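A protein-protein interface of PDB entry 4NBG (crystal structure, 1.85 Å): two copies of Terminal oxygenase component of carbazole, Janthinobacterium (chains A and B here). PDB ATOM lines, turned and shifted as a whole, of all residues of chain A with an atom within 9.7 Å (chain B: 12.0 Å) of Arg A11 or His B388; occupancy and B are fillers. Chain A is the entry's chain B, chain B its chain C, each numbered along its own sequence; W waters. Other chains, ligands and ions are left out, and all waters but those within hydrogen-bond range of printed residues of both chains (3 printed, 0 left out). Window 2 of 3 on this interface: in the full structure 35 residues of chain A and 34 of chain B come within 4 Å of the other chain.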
ATOM      1  N   VAL A   4     -28.003 -17.823  26.568  1.00  0.00           N
ATOM      2  CA  VAL A   4     -27.154 -18.901  26.078  1.00  0.00           C
ATOM      3  C   VAL A   4     -25.805 -18.416  25.556  1.00  0.00           C
ATOM      4  O   VAL A   4     -25.674 -17.279  25.108  1.00  0.00           O
ATOM      5  CB  VAL A   4     -27.873 -19.675  24.947  1.00  0.00           C
ATOM      6  CG1 VAL A   4     -26.990 -20.800  24.420  1.00  0.00           C
ATOM      7  CG2 VAL A   4     -29.191 -20.226  25.466  1.00  0.00           C
ATOM      8  N   ASP A   5     -24.810 -19.298  25.627  1.00  0.00           N
ATOM      9  CA  ASP A   5     -23.457 -19.016  25.152  1.00  0.00           C
ATOM     10  C   ASP A   5     -23.554 -18.408  23.758  1.00  0.00           C
ATOM     11  O   ASP A   5     -24.173 -18.988  22.861  1.00  0.00           O
ATOM     12  CB  ASP A   5     -22.652 -20.321  25.090  1.00  0.00           C
ATOM     13  CG  ASP A   5     -21.205 -20.107  24.671  1.00  0.00           C
ATOM     14  OD1 ASP A   5     -20.891 -19.057  24.073  1.00  0.00           O
ATOM     15  OD2 ASP A   5     -20.377 -21.006  24.930  1.00  0.00           O
ATOM     16  N   GLU A   6     -22.942 -17.243  23.577  1.00  0.00           N
ATOM     17  CA  GLU A   6     -22.974 -16.557  22.293  1.00  0.00           C
ATOM     18  C   GLU A   6     -22.414 -17.421  21.167  1.00  0.00           C
ATOM     19  O   GLU A   6     -22.813 -17.280  20.013  1.00  0.00           O
ATOM     20  CB  GLU A   6     -22.188 -15.246  22.376  1.00  0.00           C
ATOM     21  CG  GLU A   6     -22.249 -14.418  21.104  1.00  0.00           C
ATOM     22  CD  GLU A   6     -23.677 -14.146  20.655  1.00  0.00           C
ATOM     23  OE1 GLU A   6     -24.458 -13.583  21.454  1.00  0.00           O
ATOM     24  OE2 GLU A   6     -24.015 -14.496  19.502  1.00  0.00           O
ATOM     25  N   ALA A   7     -21.488 -18.311  21.508  1.00  0.00           N
ATOM     26  CA  ALA A   7     -20.878 -19.193  20.518  1.00  0.00           C
ATOM     27  C   ALA A   7     -21.931 -20.120  19.921  1.00  0.00           C
ATOM     28  O   ALA A   7     -21.906 -20.416  18.727  1.00  0.00           O
ATOM     29  CB  ALA A   7     -19.763 -20.009  21.160  1.00  0.00           C
ATOM     30  N   ILE A   8     -22.856 -20.577  20.760  1.00  0.00           N
ATOM     31  CA  ILE A   8     -23.921 -21.462  20.307  1.00  0.00           C
ATOM     32  C   ILE A   8     -24.941 -20.678  19.489  1.00  0.00           C
ATOM     33  O   ILE A   8     -25.340 -21.104  18.406  1.00  0.00           O
ATOM     34  CB  ILE A   8     -24.625 -22.148  21.501  1.00  0.00           C
ATOM     35  CG1 ILE A   8     -23.654 -23.120  22.178  1.00  0.00           C
ATOM     36  CG2 ILE A   8     -25.867 -22.892  21.028  1.00  0.00           C
ATOM     37  CD1 ILE A   8     -24.221 -23.822  23.392  1.00  0.00           C
ATOM     38  N   LEU A   9     -25.355 -19.522  19.994  1.00  0.00           N
ATOM     39  CA  LEU A   9     -26.324 -18.708  19.273  1.00  0.00           C
ATOM     40  C   LEU A   9     -25.793 -18.334  17.892  1.00  0.00           C
ATOM     41  O   LEU A   9     -26.550 -18.270  16.924  1.00  0.00           O
ATOM     42  CB  LEU A   9     -26.656 -17.444  20.073  1.00  0.00           C
ATOM     43  CG  LEU A   9     -27.336 -17.678  21.425  1.00  0.00           C
ATOM     44  CD1 LEU A   9     -27.627 -16.341  22.090  1.00  0.00           C
ATOM     45  CD2 LEU A   9     -28.633 -18.462  21.220  1.00  0.00           C
ATOM     46  N   LYS A  10     -24.490 -18.097  17.800  1.00  0.00           N
ATOM     47  CA  LYS A  10     -23.873 -17.735  16.530  1.00  0.00           C
ATOM     48  C   LYS A  10     -23.987 -18.874  15.517  1.00  0.00           C
ATOM     49  O   LYS A  10     -24.042 -18.637  14.309  1.00  0.00           O
ATOM     50  CB  LYS A  10     -22.396 -17.385  16.738  1.00  0.00           C
ATOM     51  CG  LYS A  10     -21.674 -16.961  15.466  1.00  0.00           C
ATOM     52  CD  LYS A  10     -20.206 -16.653  15.729  1.00  0.00           C
ATOM     53  CE  LYS A  10     -19.506 -16.163  14.468  1.00  0.00           C
ATOM     54  NZ  LYS A  10     -19.540 -17.178  13.376  1.00  0.00           N
ATOM     55  N   ARG A  11     -24.028 -20.106  16.019  1.00  0.00           N
ATOM     56  CA  ARG A  11     -24.129 -21.286  15.165  1.00  0.00           C
ATOM     57  C   ARG A  11     -25.527 -21.558  14.620  1.00  0.00           C
ATOM     58  O   ARG A  11     -25.670 -22.019  13.490  1.00  0.00           O
ATOM     59  CB  ARG A  11     -23.638 -22.525  15.921  1.00  0.00           C
ATOM     60  CG  ARG A  11     -22.133 -22.751  15.861  1.00  0.00           C
ATOM     61  CD  ARG A  11     -21.738 -23.942  16.718  1.00  0.00           C
ATOM     62  NE  ARG A  11     -20.368 -24.388  16.475  1.00  0.00           N
ATOM     63  CZ  ARG A  11     -19.997 -25.145  15.446  1.00  0.00           C
ATOM     64  NH1 ARG A  11     -20.896 -25.547  14.554  1.00  0.00           N
ATOM     65  NH2 ARG A  11     -18.727 -25.503  15.309  1.00  0.00           N
ATOM     66  N   VAL A  12     -26.555 -21.281  15.416  1.00  0.00           N
ATOM     67  CA  VAL A  12     -27.928 -21.523  14.978  1.00  0.00           C
ATOM     68  C   VAL A  12     -28.571 -20.265  14.402  1.00  0.00           C
ATOM     69  O   VAL A  12     -29.530 -19.731  14.954  1.00  0.00           O
ATOM     70  CB  VAL A  12     -28.790 -22.075  16.140  1.00  0.00           C
ATOM     71  CG1 VAL A  12     -28.296 -23.463  16.526  1.00  0.00           C
ATOM     72  CG2 VAL A  12     -28.719 -21.143  17.346  1.00  0.00           C
ATOM     73  N   LYS A  13     -28.040 -19.824  13.265  1.00  0.00           N
ATOM     74  CA  LYS A  13     -28.498 -18.621  12.576  1.00  0.00           C
ATOM     75  C   LYS A  13     -29.962 -18.599  12.156  1.00  0.00           C
ATOM     76  O   LYS A  13     -30.530 -17.530  11.964  1.00  0.00           O
ATOM     77  CB  LYS A  13     -27.631 -18.382  11.338  1.00  0.00           C
ATOM     78  CG  LYS A  13     -26.154 -18.198  11.641  1.00  0.00           C
ATOM     79  CD  LYS A  13     -25.345 -18.056  10.360  1.00  0.00           C
ATOM     80  CE  LYS A  13     -23.869 -17.853  10.667  1.00  0.00           C
ATOM     81  NZ  LYS A  13     -23.319 -18.983  11.466  1.00  0.00           N
ATOM     82  N   GLY A  14     -30.573 -19.770  12.005  1.00  0.00           N
ATOM     83  CA  GLY A  14     -31.961 -19.816  11.582  1.00  0.00           C
ATOM     84  C   GLY A  14     -33.007 -19.600  12.663  1.00  0.00           C
ATOM     85  O   GLY A  14     -34.153 -19.251  12.356  1.00  0.00           O
ATOM     86  N   TRP A  15     -32.630 -19.801  13.923  1.00  0.00           N
ATOM     87  CA  TRP A  15     -33.577 -19.636  15.021  1.00  0.00           C
ATOM     88  C   TRP A  15     -32.907 -19.314  16.359  1.00  0.00           C
ATOM     89  O   TRP A  15     -33.252 -19.887  17.393  1.00  0.00           O
ATOM     90  CB  TRP A  15     -34.440 -20.902  15.136  1.00  0.00           C
ATOM     91  CG  TRP A  15     -33.658 -22.198  15.110  1.00  0.00           C
ATOM     92  CD1 TRP A  15     -32.979 -22.766  16.147  1.00  0.00           C
ATOM     93  CD2 TRP A  15     -33.479 -23.075  13.986  1.00  0.00           C
ATOM     94  NE1 TRP A  15     -32.388 -23.944  15.743  1.00  0.00           N
ATOM     95  CE2 TRP A  15     -32.678 -24.156  14.422  1.00  0.00           C
ATOM     96  CE3 TRP A  15     -33.916 -23.052  12.654  1.00  0.00           C
ATOM     97  CZ2 TRP A  15     -32.303 -25.208  13.571  1.00  0.00           C
ATOM     98  CZ3 TRP A  15     -33.542 -24.099  11.807  1.00  0.00           C
ATOM     99  CH2 TRP A  15     -32.742 -25.161  12.274  1.00  0.00           C
ATOM    100  N   ALA A  16     -31.963 -18.375  16.330  1.00  0.00           N
ATOM    101  CA  ALA A  16     -31.228 -17.977  17.527  1.00  0.00           C
ATOM    102  C   ALA A  16     -32.112 -17.414  18.644  1.00  0.00           C
ATOM    103  O   ALA A  16     -31.902 -17.714  19.818  1.00  0.00           O
ATOM    104  CB  ALA A  16     -30.145 -16.969  17.158  1.00  0.00           C
ATOM    105  N   VAL A  19     -33.615 -20.336  20.512  1.00  0.00           N
ATOM    106  CA  VAL A  19     -32.659 -21.060  21.339  1.00  0.00           C
ATOM    107  C   VAL A  19     -32.325 -20.241  22.586  1.00  0.00           C
ATOM    108  O   VAL A  19     -32.083 -20.794  23.653  1.00  0.00           O
ATOM    109  CB  VAL A  19     -31.361 -21.369  20.551  1.00  0.00           C
ATOM    110  CG1 VAL A  19     -30.302 -21.945  21.483  1.00  0.00           C
ATOM    111  CG2 VAL A  19     -31.664 -22.362  19.434  1.00  0.00           C
ATOM    112  N   ASP A 347     -27.300 -26.912  26.306  1.00  0.00           N
ATOM    113  CA  ASP A 347     -27.559 -26.142  25.090  1.00  0.00           C
ATOM    114  C   ASP A 347     -26.848 -26.707  23.863  1.00  0.00           C
ATOM    115  O   ASP A 347     -27.012 -26.190  22.759  1.00  0.00           O
ATOM    116  CB  ASP A 347     -27.164 -24.667  25.267  1.00  0.00           C
ATOM    117  CG  ASP A 347     -28.007 -23.956  26.308  1.00  0.00           C
ATOM    118  OD1 ASP A 347     -29.248 -24.103  26.279  1.00  0.00           O
ATOM    119  OD2 ASP A 347     -27.429 -23.239  27.153  1.00  0.00           O
ATOM    120  N   LYS A 348     -26.073 -27.772  24.053  1.00  0.00           N
ATOM    121  CA  LYS A 348     -25.331 -28.388  22.952  1.00  0.00           C
ATOM    122  C   LYS A 348     -26.226 -29.154  21.978  1.00  0.00           C
ATOM    123  O   LYS A 348     -25.902 -29.285  20.798  1.00  0.00           O
ATOM    124  CB  LYS A 348     -24.270 -29.341  23.501  1.00  0.00           C
ATOM    125  CG  LYS A 348     -23.306 -28.714  24.493  1.00  0.00           C
ATOM    126  CD  LYS A 348     -22.276 -27.832  23.820  1.00  0.00           C
ATOM    127  CE  LYS A 348     -21.189 -27.441  24.818  1.00  0.00           C
ATOM    128  NZ  LYS A 348     -20.035 -26.767  24.166  1.00  0.00           N
ATOM    129  N   TRP A 350     -28.845 -28.270  20.652  1.00  0.00           N
ATOM    130  CA  TRP A 350     -29.323 -27.363  19.613  1.00  0.00           C
ATOM    131  C   TRP A 350     -28.348 -27.308  18.440  1.00  0.00           C
ATOM    132  O   TRP A 350     -28.670 -26.771  17.377  1.00  0.00           O
ATOM    133  CB  TRP A 350     -29.526 -25.952  20.180  1.00  0.00           C
ATOM    134  CG  TRP A 350     -30.541 -25.879  21.284  1.00  0.00           C
ATOM    135  CD1 TRP A 350     -30.302 -25.599  22.605  1.00  0.00           C
ATOM    136  CD2 TRP A 350     -31.953 -26.094  21.170  1.00  0.00           C
ATOM    137  NE1 TRP A 350     -31.478 -25.628  23.316  1.00  0.00           N
ATOM    138  CE2 TRP A 350     -32.507 -25.930  22.462  1.00  0.00           C
ATOM    139  CE3 TRP A 350     -32.804 -26.411  20.102  1.00  0.00           C
ATOM    140  CZ2 TRP A 350     -33.875 -26.073  22.714  1.00  0.00           C
ATOM    141  CZ3 TRP A 350     -34.168 -26.555  20.353  1.00  0.00           C
ATOM    142  CH2 TRP A 350     -34.688 -26.386  21.649  1.00  0.00           C
ATOM    143  N   VAL A 351     -27.152 -27.856  18.639  1.00  0.00           N
ATOM    144  CA  VAL A 351     -26.143 -27.876  17.587  1.00  0.00           C
ATOM    145  C   VAL A 351     -25.882 -29.289  17.069  1.00  0.00           C
ATOM    146  O   VAL A 351     -25.722 -29.494  15.864  1.00  0.00           O
ATOM    147  CB  VAL A 351     -24.792 -27.294  18.082  1.00  0.00           C
ATOM    148  CG1 VAL A 351     -23.713 -27.509  17.024  1.00  0.00           C
ATOM    149  CG2 VAL A 351     -24.935 -25.810  18.379  1.00  0.00           C
ATOM    150  N   ASN A 352     -25.859 -30.259  17.980  1.00  0.00           N
ATOM    151  CA  ASN A 352     -25.561 -31.646  17.622  1.00  0.00           C
ATOM    152  C   ASN A 352     -26.697 -32.546  17.140  1.00  0.00           C
ATOM    153  O   ASN A 352     -26.446 -33.643  16.638  1.00  0.00           O
ATOM    154  CB  ASN A 352     -24.843 -32.323  18.795  1.00  0.00           C
ATOM    155  CG  ASN A 352     -23.483 -31.714  19.065  1.00  0.00           C
ATOM    156  OD1 ASN A 352     -22.688 -31.532  18.145  1.00  0.00           O
ATOM    157  ND2 ASN A 352     -23.206 -31.402  20.324  1.00  0.00           N
ATOM    158  N   GLU A 353     -27.937 -32.097  17.297  1.00  0.00           N
ATOM    159  CA  GLU A 353     -29.095 -32.874  16.857  1.00  0.00           C
ATOM    160  C   GLU A 353     -28.962 -33.206  15.366  1.00  0.00           C
ATOM    161  O   GLU A 353     -28.510 -32.373  14.586  1.00  0.00           O
ATOM    162  CB  GLU A 353     -30.369 -32.050  17.069  1.00  0.00           C
ATOM    163  CG  GLU A 353     -30.355 -30.752  16.263  1.00  0.00           C
ATOM    164  CD  GLU A 353     -31.510 -29.816  16.584  1.00  0.00           C
ATOM    165  OE1 GLU A 353     -32.313 -30.127  17.488  1.00  0.00           O
ATOM    166  OE2 GLU A 353     -31.605 -28.760  15.922  1.00  0.00           O
ATOM    167  N   ALA B 380     -16.185 -32.729  25.791  1.00  0.00           N
ATOM    168  CA  ALA B 380     -16.541 -32.631  24.383  1.00  0.00           C
ATOM    169  C   ALA B 380     -16.702 -34.027  23.788  1.00  0.00           C
ATOM    170  O   ALA B 380     -17.470 -34.219  22.843  1.00  0.00           O
ATOM    171  CB  ALA B 380     -15.470 -31.852  23.622  1.00  0.00           C
ATOM    172  N   SER B 383     -20.329 -34.817  24.897  1.00  0.00           N
ATOM    173  CA  SER B 383     -21.397 -34.107  24.196  1.00  0.00           C
ATOM    174  C   SER B 383     -21.276 -34.202  22.677  1.00  0.00           C
ATOM    175  O   SER B 383     -22.279 -34.265  21.966  1.00  0.00           O
ATOM    176  CB  SER B 383     -21.418 -32.634  24.619  1.00  0.00           C
ATOM    177  OG  SER B 383     -20.205 -31.987  24.273  1.00  0.00           O
ATOM    178  N   GLY B 384     -20.042 -34.213  22.190  1.00  0.00           N
ATOM    179  CA  GLY B 384     -19.798 -34.287  20.760  1.00  0.00           C
ATOM    180  C   GLY B 384     -18.608 -33.407  20.446  1.00  0.00           C
ATOM    181  O   GLY B 384     -18.646 -32.204  20.697  1.00  0.00           O
ATOM    182  N   LEU B 385     -17.545 -34.000  19.912  1.00  0.00           N
ATOM    183  CA  LEU B 385     -16.339 -33.242  19.594  1.00  0.00           C
ATOM    184  C   LEU B 385     -16.650 -31.983  18.794  1.00  0.00           C
ATOM    185  O   LEU B 385     -17.524 -31.982  17.924  1.00  0.00           O
ATOM    186  CB  LEU B 385     -15.340 -34.126  18.846  1.00  0.00           C
ATOM    187  CG  LEU B 385     -14.746 -35.253  19.701  1.00  0.00           C
ATOM    188  CD1 LEU B 385     -13.774 -36.075  18.871  1.00  0.00           C
ATOM    189  CD2 LEU B 385     -14.036 -34.653  20.915  1.00  0.00           C
ATOM    190  N   GLU B 386     -15.921 -30.915  19.096  1.00  0.00           N
ATOM    191  CA  GLU B 386     -16.128 -29.628  18.449  1.00  0.00           C
ATOM    192  C   GLU B 386     -14.874 -29.158  17.723  1.00  0.00           C
ATOM    193  O   GLU B 386     -13.758 -29.424  18.161  1.00  0.00           O
ATOM    194  CB  GLU B 386     -16.533 -28.602  19.507  1.00  0.00           C
ATOM    195  CG  GLU B 386     -17.558 -29.135  20.498  1.00  0.00           C
ATOM    196  CD  GLU B 386     -17.901 -28.138  21.589  1.00  0.00           C
ATOM    197  OE1 GLU B 386     -16.972 -27.540  22.173  1.00  0.00           O
ATOM    198  OE2 GLU B 386     -19.104 -27.962  21.872  1.00  0.00           O
ATOM    199  N   HIS B 387     -15.069 -28.452  16.614  1.00  0.00           N
ATOM    200  CA  HIS B 387     -13.961 -27.940  15.814  1.00  0.00           C
ATOM    201  C   HIS B 387     -14.503 -26.913  14.830  1.00  0.00           C
ATOM    202  O   HIS B 387     -15.450 -27.197  14.094  1.00  0.00           O
ATOM    203  CB  HIS B 387     -13.287 -29.090  15.055  1.00  0.00           C
ATOM    204  CG  HIS B 387     -12.178 -28.655  14.148  1.00  0.00           C
ATOM    205  ND1 HIS B 387     -12.395 -27.915  13.004  1.00  0.00           N
ATOM    206  CD2 HIS B 387     -10.839 -28.857  14.216  1.00  0.00           C
ATOM    207  CE1 HIS B 387     -11.239 -27.682  12.407  1.00  0.00           C
ATOM    208  NE2 HIS B 387     -10.280 -28.241  13.123  1.00  0.00           N
ATOM    209  N   HIS B 388     -13.902 -25.724  14.818  1.00  0.00           N
ATOM    210  CA  HIS B 388     -14.347 -24.655  13.925  1.00  0.00           C
ATOM    211  C   HIS B 388     -13.403 -24.362  12.766  1.00  0.00           C
ATOM    212  O   HIS B 388     -12.185 -24.510  12.878  1.00  0.00           O
ATOM    213  CB  HIS B 388     -14.579 -23.354  14.701  1.00  0.00           C
ATOM    214  CG  HIS B 388     -15.672 -23.440  15.721  1.00  0.00           C
ATOM    215  ND1 HIS B 388     -16.362 -22.333  16.167  1.00  0.00           N
ATOM    216  CD2 HIS B 388     -16.182 -24.498  16.397  1.00  0.00           C
ATOM    217  CE1 HIS B 388     -17.251 -22.704  17.071  1.00  0.00           C
ATOM    218  NE2 HIS B 388     -17.162 -24.012  17.230  1.00  0.00           N
ATOM    219  N   HIS B 389     -14.001 -23.924  11.660  1.00  0.00           N
ATOM    220  CA  HIS B 389     -13.307 -23.568  10.420  1.00  0.00           C
ATOM    221  C   HIS B 389     -12.463 -24.693   9.834  1.00  0.00           C
ATOM    222  O   HIS B 389     -12.574 -24.929   8.614  1.00  0.00           O
ATOM    223  CB  HIS B 389     -12.456 -22.299  10.622  1.00  0.00           C
ATOM    224  CG  HIS B 389     -11.044 -22.557  11.057  1.00  0.00           C
ATOM    225  ND1 HIS B 389     -10.128 -23.224  10.271  1.00  0.00           N
ATOM    226  CD2 HIS B 389     -10.382 -22.199  12.183  1.00  0.00           C
ATOM    227  CE1 HIS B 389      -8.963 -23.264  10.893  1.00  0.00           C
ATOM    228  NE2 HIS B 389      -9.090 -22.649  12.055  1.00  0.00           N
HETATM  229  O   HOH W   1     -20.624 -30.627  21.901  1.00  0.00           O
HETATM  230  O   HOH W   2     -24.616 -32.557  22.380  1.00  0.00           O
HETATM  231  O   HOH W   3     -20.200 -30.813  17.699  1.00  0.00           O
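NE2 of His B388 is in hydrogen-bond range of NH2 of Arg A11, 2.9 Å away. The side-chain amino group of Lys A348 lies within salt-bridge range of the side-chain carboxylate of Glu B386 (2.7 Å). O of Ser B383 lies within hydrogen-bond range of ND2 of Asn A352 (3.4 Å).
The side-chain amide nitrogen (ND2) of Asn A352 is in hydrogen-bond range of the backbone carbonyl oxygen (O) of Lys A348, 3.5 Å away.
Among the printed residues, pairs that only touch across the chains: Arg A11 with His B387.
Arg A11 touches just these residues of chain B: His B387 and His B388. No residue of chain B comes within 4 Å of Ala A7. No residue of chain B comes within 4 Å of Ile A8. Val A12 touches none of the printed residues of chain B. Val A351 touches none of the printed residues of chain B. Of chain A, only Arg A11 comes within 4 Å of His B387. No residue of chain A comes within 4 Å of His B389. Printed residues of chain B within 4 Å of Lys A348: Glu B386 (2.7 Å). Printed residues of chain A within 4 Å of Ser B383: Asn A352 (3.4 Å). Of the printed residues of chain A, Glu B386 touches Lys A348. Of the printed residues of chain B, Asn A352 touches Ser B383. The nearest residue of chain B that does not touch Arg A11 is Glu B386 (5.7 Å). The nearest residue of chain A that does not touch His B388 is Ala A7 (5.4 Å).
Of the 20 printed residues of chain A, 3 touch a printed residue of chain B. Printed residues of chain A that touch a printed residue of chain B: Arg A11, Lys A348 and Asn A352. Of the 8 printed residues of chain B, 4 touch a printed residue of chain A. Hydrophobic or aromatic side chains of chain B within 4 Å of the printed part of chain A: His B388.
No position is printed for both chains. Of the 4 pairs that touch across the chains among the printed residues, none has its exchanged pair printed and touching as well.
Water W3 bridges the side-chain amide oxygen (OD1) of Asn A352 (2.6 Å) and the backbone carbonyl oxygen (O) of Leu B385 (2.9 Å). Water W2 lies within hydrogen-bond range of the side-chain amide nitrogen of Asn A352 (2.7 Å) and the backbone carbonyl oxygen of Ser B383 (2.9 Å). Water W1 lies within hydrogen-bond range of the side-chain hydroxyl (OG) of Ser B383 (2.8 Å), the backbone carbonyl oxygen (O) of Gly B384 (2.8 Å), the side-chain carboxylate (OE2) of Glu B386 (3.1 Å) and the side-chain amide nitrogen (ND2) of Asn A352 (3.1 Å).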
